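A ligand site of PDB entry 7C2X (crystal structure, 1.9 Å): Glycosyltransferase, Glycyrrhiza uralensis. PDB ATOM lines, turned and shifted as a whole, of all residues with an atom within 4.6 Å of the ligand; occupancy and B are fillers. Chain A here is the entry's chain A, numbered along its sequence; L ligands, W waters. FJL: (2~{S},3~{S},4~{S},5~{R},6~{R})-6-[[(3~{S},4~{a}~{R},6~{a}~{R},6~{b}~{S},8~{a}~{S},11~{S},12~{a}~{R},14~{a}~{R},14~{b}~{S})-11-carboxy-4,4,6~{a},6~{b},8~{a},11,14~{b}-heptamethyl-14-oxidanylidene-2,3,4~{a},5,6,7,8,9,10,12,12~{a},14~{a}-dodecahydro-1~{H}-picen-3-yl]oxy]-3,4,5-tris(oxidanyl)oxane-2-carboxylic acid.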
ATOM      1  N   PHE A  24      15.020  12.242  19.486  1.00  0.00           N
ATOM      2  CA  PHE A  24      16.119  11.604  20.205  1.00  0.00           C
ATOM      3  C   PHE A  24      15.760  11.492  21.690  1.00  0.00           C
ATOM      4  O   PHE A  24      14.681  11.921  22.107  1.00  0.00           O
ATOM      5  CB  PHE A  24      17.397  12.399  19.975  1.00  0.00           C
ATOM      6  CG  PHE A  24      18.662  11.667  20.354  1.00  0.00           C
ATOM      7  CD1 PHE A  24      18.953  10.426  19.804  1.00  0.00           C
ATOM      8  CD2 PHE A  24      19.574  12.257  21.211  1.00  0.00           C
ATOM      9  CE1 PHE A  24      20.153   9.768  20.144  1.00  0.00           C
ATOM     10  CE2 PHE A  24      20.761  11.617  21.551  1.00  0.00           C
ATOM     11  CZ  PHE A  24      21.053  10.372  21.025  1.00  0.00           C
ATOM     12  N   SER A  26      17.758  12.494  24.479  1.00  0.00           N
ATOM     13  CA  SER A  26      18.260  13.478  25.430  1.00  0.00           C
ATOM     14  C   SER A  26      17.244  14.601  25.561  1.00  0.00           C
ATOM     15  O   SER A  26      16.553  14.953  24.598  1.00  0.00           O
ATOM     16  CB  SER A  26      19.636  14.028  25.000  1.00  0.00           C
ATOM     17  OG  SER A  26      19.574  14.688  23.745  1.00  0.00           O
ATOM     18  N   HIS A  29      17.063  17.815  23.180  1.00  0.00           N
ATOM     19  CA  HIS A  29      16.700  17.410  21.824  1.00  0.00           C
ATOM     20  C   HIS A  29      15.266  16.921  21.762  1.00  0.00           C
ATOM     21  O   HIS A  29      14.526  17.212  20.807  1.00  0.00           O
ATOM     22  CB  HIS A  29      17.623  16.296  21.343  1.00  0.00           C
ATOM     23  CG  HIS A  29      18.876  16.791  20.701  1.00  0.00           C
ATOM     24  ND1 HIS A  29      19.179  16.550  19.374  1.00  0.00           N
ATOM     25  CD2 HIS A  29      19.911  17.515  21.196  1.00  0.00           C
ATOM     26  CE1 HIS A  29      20.338  17.104  19.085  1.00  0.00           C
ATOM     27  NE2 HIS A  29      20.804  17.700  20.178  1.00  0.00           N
ATOM     28  N   LEU A  93      19.064   9.984  27.978  1.00  0.00           N
ATOM     29  CA  LEU A  93      20.456  10.423  28.045  1.00  0.00           C
ATOM     30  C   LEU A  93      20.471  11.846  28.595  1.00  0.00           C
ATOM     31  O   LEU A  93      20.415  12.820  27.842  1.00  0.00           O
ATOM     32  CB  LEU A  93      21.117  10.355  26.682  1.00  0.00           C
ATOM     33  CG  LEU A  93      21.097   9.015  25.946  1.00  0.00           C
ATOM     34  CD1 LEU A  93      21.417   9.249  24.469  1.00  0.00           C
ATOM     35  CD2 LEU A  93      22.100   8.051  26.570  1.00  0.00           C
ATOM     36  N   TYR A 106      22.286   4.043  24.878  1.00  0.00           N
ATOM     37  CA  TYR A 106      22.458   4.291  23.449  1.00  0.00           C
ATOM     38  C   TYR A 106      22.389   2.986  22.665  1.00  0.00           C
ATOM     39  O   TYR A 106      21.882   2.966  21.532  1.00  0.00           O
ATOM     40  CB  TYR A 106      23.783   5.021  23.215  1.00  0.00           C
ATOM     41  CG  TYR A 106      23.990   5.553  21.806  1.00  0.00           C
ATOM     42  CD1 TYR A 106      23.247   6.628  21.322  1.00  0.00           C
ATOM     43  CD2 TYR A 106      24.940   4.991  20.970  1.00  0.00           C
ATOM     44  CE1 TYR A 106      23.445   7.118  20.024  1.00  0.00           C
ATOM     45  CE2 TYR A 106      25.153   5.476  19.690  1.00  0.00           C
ATOM     46  CZ  TYR A 106      24.407   6.531  19.220  1.00  0.00           C
ATOM     47  OH  TYR A 106      24.630   6.995  17.948  1.00  0.00           O
ATOM     48  N   MET A 132      18.723  14.509  14.112  1.00  0.00           N
ATOM     49  CA  MET A 132      20.014  14.312  13.460  1.00  0.00           C
ATOM     50  C   MET A 132      20.732  13.058  13.927  1.00  0.00           C
ATOM     51  O   MET A 132      21.566  12.513  13.193  1.00  0.00           O
ATOM     52  CB  MET A 132      20.922  15.529  13.686  1.00  0.00           C
ATOM     53  CG  MET A 132      21.114  15.833  15.186  1.00  0.00           C
ATOM     54  SD  MET A 132      21.939  17.405  15.569  1.00  0.00           S
ATOM     55  CE  MET A 132      23.482  17.111  14.682  1.00  0.00           C
ATOM     56  N   TYR A 133      20.472  12.589  15.152  1.00  0.00           N
ATOM     57  CA  TYR A 133      21.210  11.407  15.611  1.00  0.00           C
ATOM     58  C   TYR A 133      20.625  10.099  15.082  1.00  0.00           C
ATOM     59  O   TYR A 133      20.985   9.024  15.579  1.00  0.00           O
ATOM     60  CB  TYR A 133      21.294  11.393  17.146  1.00  0.00           C
ATOM     61  CG  TYR A 133      22.291  12.428  17.645  1.00  0.00           C
ATOM     62  CD1 TYR A 133      23.659  12.241  17.477  1.00  0.00           C
ATOM     63  CD2 TYR A 133      21.852  13.608  18.222  1.00  0.00           C
ATOM     64  CE1 TYR A 133      24.578  13.187  17.908  1.00  0.00           C
ATOM     65  CE2 TYR A 133      22.761  14.575  18.645  1.00  0.00           C
ATOM     66  CZ  TYR A 133      24.111  14.358  18.478  1.00  0.00           C
ATOM     67  OH  TYR A 133      25.013  15.313  18.903  1.00  0.00           O
ATOM     68  N   GLY A 153      20.088  20.629  15.925  1.00  0.00           N
ATOM     69  CA  GLY A 153      20.141  21.463  17.105  1.00  0.00           C
ATOM     70  C   GLY A 153      20.992  22.697  16.869  1.00  0.00           C
ATOM     71  O   GLY A 153      21.877  22.727  16.023  1.00  0.00           O
ATOM     72  N   GLY A 154      20.735  23.734  17.641  1.00  0.00           N
ATOM     73  CA  GLY A 154      21.649  24.844  17.641  1.00  0.00           C
ATOM     74  C   GLY A 154      21.376  25.833  16.523  1.00  0.00           C
ATOM     75  O   GLY A 154      20.373  25.795  15.831  1.00  0.00           O
ATOM     76  N   GLN A 159      26.767  26.007  12.908  1.00  0.00           N
ATOM     77  CA  GLN A 159      27.032  25.069  11.819  1.00  0.00           C
ATOM     78  C   GLN A 159      27.851  25.726  10.709  1.00  0.00           C
ATOM     79  O   GLN A 159      28.682  25.065  10.082  1.00  0.00           O
ATOM     80  CB  GLN A 159      25.716  24.499  11.287  1.00  0.00           C
ATOM     81  CG  GLN A 159      24.996  23.540  12.284  1.00  0.00           C
ATOM     82  CD  GLN A 159      25.959  22.540  12.931  1.00  0.00           C
ATOM     83  OE1 GLN A 159      26.612  21.761  12.242  1.00  0.00           O
ATOM     84  NE2 GLN A 159      26.083  22.592  14.261  1.00  0.00           N
ATOM     85  N   TRP A 200      36.625  16.979  18.746  1.00  0.00           N
ATOM     86  CA  TRP A 200      36.434  16.225  17.502  1.00  0.00           C
ATOM     87  C   TRP A 200      36.730  17.035  16.249  1.00  0.00           C
ATOM     88  O   TRP A 200      36.826  16.448  15.160  1.00  0.00           O
ATOM     89  CB  TRP A 200      35.014  15.661  17.453  1.00  0.00           C
ATOM     90  CG  TRP A 200      33.896  16.688  17.463  1.00  0.00           C
ATOM     91  CD1 TRP A 200      33.258  17.208  18.570  1.00  0.00           C
ATOM     92  CD2 TRP A 200      33.283  17.296  16.324  1.00  0.00           C
ATOM     93  NE1 TRP A 200      32.285  18.107  18.166  1.00  0.00           N
ATOM     94  CE2 TRP A 200      32.289  18.178  16.801  1.00  0.00           C
ATOM     95  CE3 TRP A 200      33.481  17.178  14.945  1.00  0.00           C
ATOM     96  CZ2 TRP A 200      31.496  18.926  15.941  1.00  0.00           C
ATOM     97  CZ3 TRP A 200      32.691  17.934  14.091  1.00  0.00           C
ATOM     98  CH2 TRP A 200      31.713  18.795  14.591  1.00  0.00           C
ATOM     99  N   GLU A 207      36.067   9.316  17.627  1.00  0.00           N
ATOM    100  CA  GLU A 207      34.863   8.560  17.282  1.00  0.00           C
ATOM    101  C   GLU A 207      33.689   9.500  16.993  1.00  0.00           C
ATOM    102  O   GLU A 207      32.871   9.217  16.125  1.00  0.00           O
ATOM    103  CB  GLU A 207      34.521   7.567  18.382  1.00  0.00           C
ATOM    104  CG  GLU A 207      35.278   6.241  18.255  1.00  0.00           C
ATOM    105  CD  GLU A 207      35.330   5.724  16.807  1.00  0.00           C
ATOM    106  OE1 GLU A 207      36.341   5.971  16.111  1.00  0.00           O
ATOM    107  OE2 GLU A 207      34.345   5.079  16.373  1.00  0.00           O
ATOM    108  N   TYR A 208      33.631  10.637  17.684  1.00  0.00           N
ATOM    109  CA  TYR A 208      32.568  11.597  17.415  1.00  0.00           C
ATOM    110  C   TYR A 208      32.760  12.303  16.073  1.00  0.00           C
ATOM    111  O   TYR A 208      31.774  12.654  15.424  1.00  0.00           O
ATOM    112  CB  TYR A 208      32.478  12.614  18.548  1.00  0.00           C
ATOM    113  CG  TYR A 208      31.194  13.426  18.545  1.00  0.00           C
ATOM    114  CD1 TYR A 208      30.027  12.914  19.104  1.00  0.00           C
ATOM    115  CD2 TYR A 208      31.151  14.693  17.987  1.00  0.00           C
ATOM    116  CE1 TYR A 208      28.852  13.646  19.102  1.00  0.00           C
ATOM    117  CE2 TYR A 208      30.000  15.444  17.981  1.00  0.00           C
ATOM    118  CZ  TYR A 208      28.844  14.906  18.535  1.00  0.00           C
ATOM    119  OH  TYR A 208      27.675  15.667  18.524  1.00  0.00           O
ATOM    120  N   LEU A 211      31.038  10.003  13.674  1.00  0.00           N
ATOM    121  CA  LEU A 211      29.588  10.126  13.796  1.00  0.00           C
ATOM    122  C   LEU A 211      29.084  11.385  13.095  1.00  0.00           C
ATOM    123  O   LEU A 211      28.095  11.353  12.364  1.00  0.00           O
ATOM    124  CB  LEU A 211      29.168  10.125  15.258  1.00  0.00           C
ATOM    125  CG  LEU A 211      27.672  10.325  15.521  1.00  0.00           C
ATOM    126  CD1 LEU A 211      26.820   9.320  14.712  1.00  0.00           C
ATOM    127  CD2 LEU A 211      27.367  10.204  17.007  1.00  0.00           C
ATOM    128  N   MET A 301      22.167  19.361  30.678  1.00  0.00           N
ATOM    129  CA  MET A 301      23.208  18.324  30.671  1.00  0.00           C
ATOM    130  C   MET A 301      24.397  18.609  31.570  1.00  0.00           C
ATOM    131  O   MET A 301      25.186  17.685  31.828  1.00  0.00           O
ATOM    132  CB  MET A 301      23.746  18.110  29.240  1.00  0.00           C
ATOM    133  CG  MET A 301      22.660  17.867  28.196  1.00  0.00           C
ATOM    134  SD  MET A 301      21.697  16.375  28.551  1.00  0.00           S
ATOM    135  CE  MET A 301      23.006  15.173  28.763  1.00  0.00           C
ATOM    136  N   ALA A 400      29.763  21.078  23.522  1.00  0.00           N
ATOM    137  CA  ALA A 400      28.960  21.008  22.292  1.00  0.00           C
ATOM    138  C   ALA A 400      29.326  22.201  21.412  1.00  0.00           C
ATOM    139  O   ALA A 400      30.519  22.480  21.241  1.00  0.00           O
ATOM    140  CB  ALA A 400      27.483  20.880  22.667  1.00  0.00           C
ATOM    141  N   GLU A 401      28.349  22.934  20.861  1.00  0.00           N
ATOM    142  CA  GLU A 401      28.575  24.056  19.960  1.00  0.00           C
ATOM    143  C   GLU A 401      28.472  25.403  20.681  1.00  0.00           C
ATOM    144  O   GLU A 401      28.370  26.448  20.019  1.00  0.00           O
ATOM    145  CB  GLU A 401      27.575  23.968  18.798  1.00  0.00           C
ATOM    146  CG  GLU A 401      26.196  24.669  19.025  1.00  0.00           C
ATOM    147  CD  GLU A 401      25.227  23.968  19.998  1.00  0.00           C
ATOM    148  OE1 GLU A 401      25.605  22.952  20.626  1.00  0.00           O
ATOM    149  OE2 GLU A 401      24.066  24.460  20.131  1.00  0.00           O
ATOM    150  N   ASN A 426      34.636  18.324  27.336  1.00  0.00           N
ATOM    151  CA  ASN A 426      33.540  17.420  27.022  1.00  0.00           C
ATOM    152  C   ASN A 426      32.463  17.522  28.089  1.00  0.00           C
ATOM    153  O   ASN A 426      32.672  18.030  29.200  1.00  0.00           O
ATOM    154  CB  ASN A 426      34.022  15.974  26.876  1.00  0.00           C
ATOM    155  CG  ASN A 426      33.694  15.398  25.514  1.00  0.00           C
ATOM    156  OD1 ASN A 426      32.619  15.655  24.947  1.00  0.00           O
ATOM    157  ND2 ASN A 426      34.630  14.642  24.952  1.00  0.00           N
ATOM    158  N   TRP A 427      31.278  17.043  27.728  1.00  0.00           N
ATOM    159  CA  TRP A 427      30.137  17.192  28.623  1.00  0.00           C
ATOM    160  C   TRP A 427      30.261  16.295  29.859  1.00  0.00           C
ATOM    161  O   TRP A 427      29.582  16.562  30.860  1.00  0.00           O
ATOM    162  CB  TRP A 427      28.863  16.868  27.856  1.00  0.00           C
ATOM    163  CG  TRP A 427      28.587  15.429  27.876  1.00  0.00           C
ATOM    164  CD1 TRP A 427      29.213  14.459  27.151  1.00  0.00           C
ATOM    165  CD2 TRP A 427      27.638  14.773  28.709  1.00  0.00           C
ATOM    166  NE1 TRP A 427      28.692  13.228  27.480  1.00  0.00           N
ATOM    167  CE2 TRP A 427      27.722  13.391  28.425  1.00  0.00           C
ATOM    168  CE3 TRP A 427      26.710  15.220  29.653  1.00  0.00           C
ATOM    169  CZ2 TRP A 427      26.922  12.456  29.060  1.00  0.00           C
ATOM    170  CZ3 TRP A 427      25.907  14.277  30.283  1.00  0.00           C
ATOM    171  CH2 TRP A 427      26.010  12.922  29.984  1.00  0.00           C
HETATM  172  C11 FJL L   1      26.041  11.778  23.670  1.00  0.00           C
HETATM  173  C12 FJL L   1      26.330  14.475  23.484  1.00  0.00           C
HETATM  174  C13 FJL L   1      26.853  13.017  23.137  1.00  0.00           C
HETATM  175  C14 FJL L   1      26.546  10.504  22.809  1.00  0.00           C
HETATM  176  C15 FJL L   1      24.812  14.508  23.104  1.00  0.00           C
HETATM  177  C16 FJL L   1      24.508  12.025  23.509  1.00  0.00           C
HETATM  178  C17 FJL L   1      24.120  15.967  23.020  1.00  0.00           C
HETATM  179  C18 FJL L   1      24.086  13.448  23.968  1.00  0.00           C
HETATM  180  C19 FJL L   1      28.052  10.252  23.015  1.00  0.00           C
HETATM  181  C20 FJL L   1      28.712   8.903  22.570  1.00  0.00           C
HETATM  182  C21 FJL L   1      27.880   7.716  23.152  1.00  0.00           C
HETATM  183  C22 FJL L   1      25.830   9.215  23.325  1.00  0.00           C
HETATM  184  C23 FJL L   1      27.095  15.565  22.666  1.00  0.00           C
HETATM  185  C24 FJL L   1      26.426   7.942  22.683  1.00  0.00           C
HETATM  186  C25 FJL L   1      25.052  16.927  22.151  1.00  0.00           C
HETATM  187  C26 FJL L   1      28.319  12.694  23.339  1.00  0.00           C
HETATM  188  C27 FJL L   1      26.277  11.508  25.165  1.00  0.00           C
HETATM  189  C28 FJL L   1      26.463  16.962  22.782  1.00  0.00           C
HETATM  190  C29 FJL L   1      26.609  14.796  24.965  1.00  0.00           C
HETATM  191  C30 FJL L   1      26.134  10.703  21.335  1.00  0.00           C
HETATM  192  C31 FJL L   1      28.847  11.325  23.143  1.00  0.00           C
HETATM  193  C32 FJL L   1      28.955   8.741  21.038  1.00  0.00           C
HETATM  194  C33 FJL L   1      28.440   6.334  22.663  1.00  0.00           C
HETATM  195  C34 FJL L   1      29.701   7.420  20.676  1.00  0.00           C
HETATM  196  C35 FJL L   1      23.837  16.564  24.402  1.00  0.00           C
HETATM  197  C36 FJL L   1      22.776  15.810  22.287  1.00  0.00           C
HETATM  198  C37 FJL L   1      28.811   6.257  21.176  1.00  0.00           C
HETATM  199  C38 FJL L   1      27.928   7.730  24.704  1.00  0.00           C
HETATM  200  C39 FJL L   1      29.902   7.311  19.145  1.00  0.00           C
HETATM  201  C40 FJL L   1      31.149   7.386  21.335  1.00  0.00           C
HETATM  202  C41 FJL L   1      24.449  18.633  20.592  1.00  0.00           C
HETATM  203  C42 FJL L   1      23.775  20.072  20.412  1.00  0.00           C
HETATM  204  C43 FJL L   1      23.822  20.394  18.862  1.00  0.00           C
HETATM  205  C44 FJL L   1      25.963  18.983  18.789  1.00  0.00           C
HETATM  206  C45 FJL L   1      25.318  20.350  18.375  1.00  0.00           C
HETATM  207  C46 FJL L   1      27.555  18.979  18.456  1.00  0.00           C
HETATM  208  O01 FJL L   1      24.507  18.241  21.974  1.00  0.00           O
HETATM  209  O02 FJL L   1      29.133  13.598  23.683  1.00  0.00           O
HETATM  210  O03 FJL L   1      31.446   6.487  22.140  1.00  0.00           O
HETATM  211  O04 FJL L   1      25.792  18.775  20.176  1.00  0.00           O
HETATM  212  O05 FJL L   1      31.947   8.294  20.978  1.00  0.00           O
HETATM  213  O06 FJL L   1      22.449  19.920  20.834  1.00  0.00           O
HETATM  214  O07 FJL L   1      23.301  21.698  18.707  1.00  0.00           O
HETATM  215  O08 FJL L   1      25.304  20.475  16.974  1.00  0.00           O
HETATM  216  O09 FJL L   1      28.234  18.171  19.106  1.00  0.00           O
HETATM  217  O10 FJL L   1      27.967  19.787  17.605  1.00  0.00           O
HETATM  218  O   HOH W   1      23.302  20.550  15.135  1.00  0.00           O
HETATM  219  O   HOH W   2      30.458  17.731  21.017  1.00  0.00           O
HETATM  220  O   HOH W   3      21.599  19.162  23.743  1.00  0.00           O
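N of Gly 154 lies within hydrogen-bond range of O07 of the ligand. OE2 of Glu 401 is in hydrogen-bond range of O07 of the ligand (3.2 Å). A ring nitrogen (NE2) of His 29 sits at hydrogen-bond distance from an oxygen (O06) of the ligand. The backbone carbonyl oxygen (O) of Gly 153 lies close to an oxygen (O07) of the ligand (3.2 Å). The side-chain hydroxyl (OH) of Tyr 208 is in hydrogen-bond range of an oxygen (O09) of the ligand (2.6 Å).
Residues that only touch the ligand: Ser 26 (3.7 Å), Tyr 106 (3.5 Å), Tyr 133 (3.6 Å), Gln 159 (3.5 Å), Trp 200 (3.996 Å), Glu 207 (3.7 Å), Ala 400 (3.7 Å) and Trp 427 (3.4 Å). Hydrophobic or aromatic side chains within 4 Å of the ligand: His 29, Tyr 106, Tyr 133, Trp 200, Tyr 208, Ala 400 and Trp 427. Of the 19 residues printed, 13 come within 4 Å of the ligand. The nearest printed residue that does not touch the ligand is Met 301 (4.2 Å).
Water W1 lies within hydrogen-bond range of O08 of the ligand (2.7 Å), O of Gly 153 (2.7 Å) and SD of Met 132 (3.5 Å). Water W2 lies within hydrogen-bond range of an oxygen (O09) of the ligand (3.0 Å) and the indole nitrogen (NE1) of Trp 200 (3.4 Å).
The side-chain sulfur of Met 132 is in hydrogen-bond range of the backbone NH of Gly 153 (3.7 Å). The side-chain hydroxyl of Tyr 208 lies within hydrogen-bond range of the side-chain hydroxyl of Tyr 133 (2.7 Å).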
